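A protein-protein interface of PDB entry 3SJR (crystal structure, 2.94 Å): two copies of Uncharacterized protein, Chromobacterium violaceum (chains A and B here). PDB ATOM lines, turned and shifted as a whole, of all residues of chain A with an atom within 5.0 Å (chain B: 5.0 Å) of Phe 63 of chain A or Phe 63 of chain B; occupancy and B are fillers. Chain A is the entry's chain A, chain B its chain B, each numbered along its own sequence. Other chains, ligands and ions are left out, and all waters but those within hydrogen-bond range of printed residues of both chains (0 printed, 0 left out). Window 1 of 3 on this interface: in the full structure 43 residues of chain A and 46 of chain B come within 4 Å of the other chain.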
ATOM      1  N   ALA A  59      26.337  11.457 -19.100  1.00  0.00           N
ATOM      2  CA  ALA A  59      25.455  12.110 -18.157  1.00  0.00           C
ATOM      3  C   ALA A  59      25.501  11.446 -16.793  1.00  0.00           C
ATOM      4  O   ALA A  59      25.392  12.119 -15.783  1.00  0.00           O
ATOM      5  CB  ALA A  59      24.041  12.112 -18.692  1.00  0.00           C
ATOM      6  N   ALA A  60      25.670  10.127 -16.768  1.00  0.00           N
ATOM      7  CA  ALA A  60      25.618   9.371 -15.522  1.00  0.00           C
ATOM      8  C   ALA A  60      26.846   9.697 -14.726  1.00  0.00           C
ATOM      9  O   ALA A  60      26.759  10.031 -13.547  1.00  0.00           O
ATOM     10  CB  ALA A  60      25.547   7.917 -15.792  1.00  0.00           C
ATOM     11  N   LEU A  61      27.991   9.632 -15.391  1.00  0.00           N
ATOM     12  CA  LEU A  61      29.257   9.997 -14.778  1.00  0.00           C
ATOM     13  C   LEU A  61      29.225  11.391 -14.148  1.00  0.00           C
ATOM     14  O   LEU A  61      29.614  11.564 -13.000  1.00  0.00           O
ATOM     15  CB  LEU A  61      30.377   9.884 -15.805  1.00  0.00           C
ATOM     16  CG  LEU A  61      30.742   8.437 -16.153  1.00  0.00           C
ATOM     17  CD1 LEU A  61      31.645   8.399 -17.373  1.00  0.00           C
ATOM     18  CD2 LEU A  61      31.404   7.734 -14.978  1.00  0.00           C
ATOM     19  N   LEU A  62      28.743  12.375 -14.900  1.00  0.00           N
ATOM     20  CA  LEU A  62      28.541  13.720 -14.377  1.00  0.00           C
ATOM     21  C   LEU A  62      27.582  13.712 -13.175  1.00  0.00           C
ATOM     22  O   LEU A  62      27.856  14.335 -12.136  1.00  0.00           O
ATOM     23  CB  LEU A  62      28.009  14.638 -15.482  1.00  0.00           C
ATOM     24  CG  LEU A  62      27.945  16.151 -15.221  1.00  0.00           C
ATOM     25  CD1 LEU A  62      29.268  16.721 -14.774  1.00  0.00           C
ATOM     26  CD2 LEU A  62      27.484  16.887 -16.460  1.00  0.00           C
ATOM     27  N   PHE A  63      26.472  12.985 -13.301  1.00  0.00           N
ATOM     28  CA  PHE A  63      25.476  12.981 -12.239  1.00  0.00           C
ATOM     29  C   PHE A  63      26.110  12.503 -10.959  1.00  0.00           C
ATOM     30  O   PHE A  63      26.049  13.180  -9.934  1.00  0.00           O
ATOM     31  CB  PHE A  63      24.274  12.098 -12.560  1.00  0.00           C
ATOM     32  CG  PHE A  63      23.156  12.269 -11.586  1.00  0.00           C
ATOM     33  CD1 PHE A  63      23.033  11.430 -10.496  1.00  0.00           C
ATOM     34  CD2 PHE A  63      22.252  13.298 -11.730  1.00  0.00           C
ATOM     35  CE1 PHE A  63      22.002  11.596  -9.581  1.00  0.00           C
ATOM     36  CE2 PHE A  63      21.221  13.472 -10.826  1.00  0.00           C
ATOM     37  CZ  PHE A  63      21.100  12.620  -9.745  1.00  0.00           C
ATOM     38  N   SER A  64      26.721  11.328 -11.049  1.00  0.00           N
ATOM     39  CA  SER A  64      27.258  10.649  -9.899  1.00  0.00           C
ATOM     40  C   SER A  64      28.406  11.445  -9.279  1.00  0.00           C
ATOM     41  O   SER A  64      28.527  11.518  -8.054  1.00  0.00           O
ATOM     42  CB  SER A  64      27.706   9.238 -10.287  1.00  0.00           C
ATOM     43  OG  SER A  64      28.009   8.461  -9.141  1.00  0.00           O
ATOM     44  N   ALA A  65      29.240  12.062 -10.110  1.00  0.00           N
ATOM     45  CA  ALA A  65      30.393  12.729  -9.567  1.00  0.00           C
ATOM     46  C   ALA A  65      29.904  13.971  -8.859  1.00  0.00           C
ATOM     47  O   ALA A  65      30.298  14.233  -7.719  1.00  0.00           O
ATOM     48  CB  ALA A  65      31.385  13.048 -10.634  1.00  0.00           C
ATOM     49  N   ALA A  66      29.004  14.702  -9.512  1.00  0.00           N
ATOM     50  CA  ALA A  66      28.533  15.988  -8.993  1.00  0.00           C
ATOM     51  C   ALA A  66      27.751  15.832  -7.698  1.00  0.00           C
ATOM     52  O   ALA A  66      27.970  16.549  -6.728  1.00  0.00           O
ATOM     53  CB  ALA A  66      27.705  16.705 -10.032  1.00  0.00           C
ATOM     54  N   MET A  67      26.851  14.866  -7.688  1.00  0.00           N
ATOM     55  CA  MET A  67      26.019  14.616  -6.543  1.00  0.00           C
ATOM     56  C   MET A  67      26.936  14.361  -5.364  1.00  0.00           C
ATOM     57  O   MET A  67      26.668  14.813  -4.257  1.00  0.00           O
ATOM     58  CB  MET A  67      25.092  13.435  -6.830  1.00  0.00           C
ATOM     59  CG  MET A  67      23.617  13.740  -6.635  1.00  0.00           C
ATOM     60  SD  MET A  67      23.046  15.508  -7.244  1.00  0.00           S
ATOM     61  CE  MET A  67      23.883  15.599  -9.007  1.00  0.00           C
ATOM     62  N   ASP A  68      28.047  13.686  -5.619  1.00  0.00           N
ATOM     63  CA  ASP A  68      29.054  13.478  -4.586  1.00  0.00           C
ATOM     64  C   ASP A  68      29.696  14.796  -4.164  1.00  0.00           C
ATOM     65  O   ASP A  68      29.660  15.185  -2.989  1.00  0.00           O
ATOM     66  CB  ASP A  68      30.137  12.515  -5.084  1.00  0.00           C
ATOM     67  CG  ASP A  68      31.187  12.212  -4.032  1.00  0.00           C
ATOM     68  OD1 ASP A  68      31.027  12.593  -2.845  1.00  0.00           O
ATOM     69  OD2 ASP A  68      32.191  11.583  -4.410  1.00  0.00           O
ATOM     70  N   HIS A  96      28.134   5.152  -1.346  1.00  0.00           N
ATOM     71  CA  HIS A  96      27.615   6.238  -2.161  1.00  0.00           C
ATOM     72  C   HIS A  96      26.127   5.957  -2.331  1.00  0.00           C
ATOM     73  O   HIS A  96      25.285   6.764  -1.935  1.00  0.00           O
ATOM     74  CB  HIS A  96      28.364   6.248  -3.509  1.00  0.00           C
ATOM     75  CG  HIS A  96      28.038   7.406  -4.415  1.00  0.00           C
ATOM     76  ND1 HIS A  96      27.912   8.708  -3.968  1.00  0.00           N
ATOM     77  CD2 HIS A  96      27.880   7.459  -5.760  1.00  0.00           C
ATOM     78  CE1 HIS A  96      27.652   9.503  -4.994  1.00  0.00           C
ATOM     79  NE2 HIS A  96      27.624   8.770  -6.092  1.00  0.00           N
ATOM     80  N   LEU A  97      25.825   4.769  -2.859  1.00  0.00           N
ATOM     81  CA  LEU A  97      24.465   4.330  -3.126  1.00  0.00           C
ATOM     82  C   LEU A  97      23.548   4.460  -1.922  1.00  0.00           C
ATOM     83  O   LEU A  97      22.475   5.035  -2.029  1.00  0.00           O
ATOM     84  CB  LEU A  97      24.489   2.899  -3.617  1.00  0.00           C
ATOM     85  CG  LEU A  97      24.545   2.714  -5.133  1.00  0.00           C
ATOM     86  CD1 LEU A  97      25.342   1.480  -5.531  1.00  0.00           C
ATOM     87  CD2 LEU A  97      23.129   2.601  -5.669  1.00  0.00           C
ATOM     88  N   GLY A 100      22.860   7.905  -0.967  1.00  0.00           N
ATOM     89  CA  GLY A 100      21.911   8.426  -1.932  1.00  0.00           C
ATOM     90  C   GLY A 100      20.492   8.155  -1.483  1.00  0.00           C
ATOM     91  O   GLY A 100      19.642   9.061  -1.453  1.00  0.00           O
ATOM     92  N   ALA B  59      29.296   1.623 -11.622  1.00  0.00           N
ATOM     93  CA  ALA B  59      28.752   2.085 -10.358  1.00  0.00           C
ATOM     94  C   ALA B  59      28.034   3.383 -10.588  1.00  0.00           C
ATOM     95  O   ALA B  59      26.933   3.576 -10.105  1.00  0.00           O
ATOM     96  CB  ALA B  59      29.846   2.268  -9.341  1.00  0.00           C
ATOM     97  N   ALA B  60      28.667   4.269 -11.346  1.00  0.00           N
ATOM     98  CA  ALA B  60      28.090   5.566 -11.639  1.00  0.00           C
ATOM     99  C   ALA B  60      26.776   5.390 -12.378  1.00  0.00           C
ATOM    100  O   ALA B  60      25.791   6.015 -12.038  1.00  0.00           O
ATOM    101  CB  ALA B  60      29.048   6.409 -12.420  1.00  0.00           C
ATOM    102  N   LEU B  61      26.754   4.518 -13.369  1.00  0.00           N
ATOM    103  CA  LEU B  61      25.509   4.164 -14.043  1.00  0.00           C
ATOM    104  C   LEU B  61      24.404   3.808 -13.055  1.00  0.00           C
ATOM    105  O   LEU B  61      23.338   4.443 -13.053  1.00  0.00           O
ATOM    106  CB  LEU B  61      25.735   3.006 -15.025  1.00  0.00           C
ATOM    107  CG  LEU B  61      26.530   3.449 -16.260  1.00  0.00           C
ATOM    108  CD1 LEU B  61      26.795   2.280 -17.201  1.00  0.00           C
ATOM    109  CD2 LEU B  61      25.841   4.602 -17.024  1.00  0.00           C
ATOM    110  N   LEU B  62      24.680   2.800 -12.218  1.00  0.00           N
ATOM    111  CA  LEU B  62      23.719   2.300 -11.250  1.00  0.00           C
ATOM    112  C   LEU B  62      23.306   3.432 -10.339  1.00  0.00           C
ATOM    113  O   LEU B  62      22.114   3.617 -10.096  1.00  0.00           O
ATOM    114  CB  LEU B  62      24.281   1.122 -10.453  1.00  0.00           C
ATOM    115  CG  LEU B  62      23.508   0.483  -9.272  1.00  0.00           C
ATOM    116  CD1 LEU B  62      22.112   0.029  -9.616  1.00  0.00           C
ATOM    117  CD2 LEU B  62      24.266  -0.689  -8.679  1.00  0.00           C
ATOM    118  N   PHE B  63      24.269   4.209  -9.856  1.00  0.00           N
ATOM    119  CA  PHE B  63      23.918   5.313  -9.004  1.00  0.00           C
ATOM    120  C   PHE B  63      22.898   6.208  -9.720  1.00  0.00           C
ATOM    121  O   PHE B  63      21.753   6.351  -9.259  1.00  0.00           O
ATOM    122  CB  PHE B  63      25.130   6.120  -8.565  1.00  0.00           C
ATOM    123  CG  PHE B  63      24.769   7.226  -7.636  1.00  0.00           C
ATOM    124  CD1 PHE B  63      24.415   8.473  -8.124  1.00  0.00           C
ATOM    125  CD2 PHE B  63      24.715   7.011  -6.274  1.00  0.00           C
ATOM    126  CE1 PHE B  63      24.043   9.502  -7.264  1.00  0.00           C
ATOM    127  CE2 PHE B  63      24.351   8.044  -5.396  1.00  0.00           C
ATOM    128  CZ  PHE B  63      24.003   9.287  -5.896  1.00  0.00           C
ATOM    129  N   SER B  64      23.309   6.803 -10.841  1.00  0.00           N
ATOM    130  CA  SER B  64      22.482   7.803 -11.512  1.00  0.00           C
ATOM    131  C   SER B  64      21.072   7.254 -11.721  1.00  0.00           C
ATOM    132  O   SER B  64      20.105   7.786 -11.169  1.00  0.00           O
ATOM    133  CB  SER B  64      23.110   8.254 -12.832  1.00  0.00           C
ATOM    134  OG  SER B  64      22.196   9.015 -13.608  1.00  0.00           O
ATOM    135  N   ALA B  65      20.975   6.167 -12.483  1.00  0.00           N
ATOM    136  CA  ALA B  65      19.716   5.495 -12.753  1.00  0.00           C
ATOM    137  C   ALA B  65      18.891   5.299 -11.484  1.00  0.00           C
ATOM    138  O   ALA B  65      17.733   5.688 -11.427  1.00  0.00           O
ATOM    139  CB  ALA B  65      19.972   4.157 -13.453  1.00  0.00           C
ATOM    140  N   ALA B  66      19.476   4.711 -10.455  1.00  0.00           N
ATOM    141  CA  ALA B  66      18.682   4.387  -9.279  1.00  0.00           C
ATOM    142  C   ALA B  66      18.131   5.646  -8.616  1.00  0.00           C
ATOM    143  O   ALA B  66      17.006   5.676  -8.145  1.00  0.00           O
ATOM    144  CB  ALA B  66      19.477   3.551  -8.300  1.00  0.00           C
ATOM    145  N   MET B  67      18.921   6.703  -8.603  1.00  0.00           N
ATOM    146  CA  MET B  67      18.455   7.950  -8.042  1.00  0.00           C
ATOM    147  C   MET B  67      17.314   8.477  -8.892  1.00  0.00           C
ATOM    148  O   MET B  67      16.323   8.994  -8.379  1.00  0.00           O
ATOM    149  CB  MET B  67      19.614   8.934  -7.960  1.00  0.00           C
ATOM    150  CG  MET B  67      20.723   8.379  -7.115  1.00  0.00           C
ATOM    151  SD  MET B  67      20.024   8.185  -5.319  1.00  0.00           S
ATOM    152  CE  MET B  67      19.906  10.088  -4.917  1.00  0.00           C
ATOM    153  N   ASP B  68      17.455   8.312 -10.201  1.00  0.00           N
ATOM    154  CA  ASP B  68      16.400   8.676 -11.130  1.00  0.00           C
ATOM    155  C   ASP B  68      15.132   7.918 -10.748  1.00  0.00           C
ATOM    156  O   ASP B  68      14.143   8.502 -10.303  1.00  0.00           O
ATOM    157  CB  ASP B  68      16.814   8.343 -12.563  1.00  0.00           C
ATOM    158  CG  ASP B  68      15.817   8.824 -13.567  1.00  0.00           C
ATOM    159  OD1 ASP B  68      15.710  10.057 -13.719  1.00  0.00           O
ATOM    160  OD2 ASP B  68      15.128   7.982 -14.191  1.00  0.00           O
ATOM    161  N   HIS B  96      17.615  15.787 -15.015  1.00  0.00           N
ATOM    162  CA  HIS B  96      18.101  14.857 -14.019  1.00  0.00           C
ATOM    163  C   HIS B  96      19.011  15.630 -13.070  1.00  0.00           C
ATOM    164  O   HIS B  96      18.700  15.762 -11.882  1.00  0.00           O
ATOM    165  CB  HIS B  96      18.782  13.638 -14.688  1.00  0.00           C
ATOM    166  CG  HIS B  96      19.156  12.533 -13.734  1.00  0.00           C
ATOM    167  ND1 HIS B  96      18.389  12.194 -12.634  1.00  0.00           N
ATOM    168  CD2 HIS B  96      20.217  11.687 -13.722  1.00  0.00           C
ATOM    169  CE1 HIS B  96      18.974  11.206 -11.978  1.00  0.00           C
ATOM    170  NE2 HIS B  96      20.085  10.882 -12.616  1.00  0.00           N
ATOM    171  N   LEU B  97      20.091  16.188 -13.611  1.00  0.00           N
ATOM    172  CA  LEU B  97      21.036  17.007 -12.856  1.00  0.00           C
ATOM    173  C   LEU B  97      20.400  18.119 -12.039  1.00  0.00           C
ATOM    174  O   LEU B  97      20.789  18.368 -10.899  1.00  0.00           O
ATOM    175  CB  LEU B  97      22.017  17.637 -13.820  1.00  0.00           C
ATOM    176  CG  LEU B  97      23.288  16.846 -14.056  1.00  0.00           C
ATOM    177  CD1 LEU B  97      24.034  17.403 -15.230  1.00  0.00           C
ATOM    178  CD2 LEU B  97      24.133  16.947 -12.813  1.00  0.00           C
ATOM    179  N   GLY B 100      18.599  16.798  -9.307  1.00  0.00           N
ATOM    180  CA  GLY B 100      19.648  16.435  -8.369  1.00  0.00           C
ATOM    181  C   GLY B 100      19.907  17.570  -7.407  1.00  0.00           C
ATOM    182  O   GLY B 100      19.680  17.432  -6.199  1.00  0.00           O
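Ser 64 of chain B touches Ala 60 of chain A (CB to CA, 3.8 Å).
CD2 of Leu 61 of chain A touches CB of Ala 60 of chain B, 3.7 Å away.
Ser 64 of chain B touches Phe 63 of chain A (CA to CD1, 3.8 Å).
Met 67 of chain B touches Phe 63 of chain A (CB to CE1, 3.9 Å).
CD2 of Phe 63 of chain A touches CD2 of His 96 of chain B, 3.3 Å away.
CB of Ser 64 of chain A touches CB of Ala 60 of chain B, 3.8 Å away.
Met 67 of chain A touches Gly 100 of chain B (SD to CA, 3.7 Å).
CD2 of His 96 of chain A touches CD2 of Phe 63 of chain B, 3.2 Å away.
Leu 97 of chain A touches Leu 62 of chain B.
Gly 100 of chain A touches Met 67 of chain B (O to CE, 3.6 Å).
Of the 13 printed residues of chain B, 9 touch a printed residue of chain A.
Hydrophobic or aromatic side chains of chain A within 4 Å of the printed part of chain B: Ala 60, Leu 61, Leu 62, Phe 63, Met 67, His 96 and Leu 97.
Among the printed residues, 14 pairs touch across the chains.
Among the printed residues, no Asp or Glu carboxylate lies within 4 Å of a Lys or Arg side-chain nitrogen of the other chain.
Phe 63 of chain A touches Ser 64 of chain B, and with the chains exchanged Ser 64 of chain A touches Phe 63 of chain B.
Phe 63 of chain A touches Met 67 of chain B, but with the chains exchanged Met 67 of chain A does not touch Phe 63 of chain B (4.1 Å).
Phe 63 of chain A touches His 96 of chain B, and with the chains exchanged His 96 of chain A touches Phe 63 of chain B.
Met 67 of chain A touches Gly 100 of chain B, and with the chains exchanged Gly 100 of chain A touches Met 67 of chain B.
13 positions are printed for both chains.
Of the 14 pairs that touch across the chains among the printed residues, 13 have their exchanged pair printed and touching as well.
Of chain B, only Phe 63 (3.7 Å), Ser 64 (3.8 Å), Met 67 (3.9 Å) and His 96 (3.3 Å) come within 4 Å of Phe 63 of chain A.
Of the printed residues of chain B, His 96 of chain A touches Phe 63 (3.2 Å).
Of the printed residues of chain B, Ala 60 of chain A touches Leu 61 and Ser 64.
Printed residues of chain A within 4 Å of Leu 97 of chain B: Leu 62 (3.7 Å).
Printed residues of chain B within 4 Å of Leu 62 of chain A: Leu 97 (3.7 Å).
Asp 68 of chain B touches none of the printed residues of chain A.
Ala 59 of chain A touches none of the printed residues of chain B.
The nearest residue of chain B that does not touch Phe 63 of chain A is Leu 97 of chain B (4.1 Å).
The nearest residue of chain A that does not touch Phe 63 of chain B is Met 67 of chain A (4.1 Å).
The nearest printed residue of chain A that does not touch Leu 97 of chain B is Met 67 of chain A (4.05 Å).
The side-chain hydroxyl (OG) of Ser 64 of chain B lies within hydrogen-bond range of a ring nitrogen (NE2) of His 96 of chain B (3.0 Å).
A ring nitrogen (NE2) of His 96 of chain A lies within hydrogen-bond range of the side-chain hydroxyl (OG) of Ser 64 of chain A.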
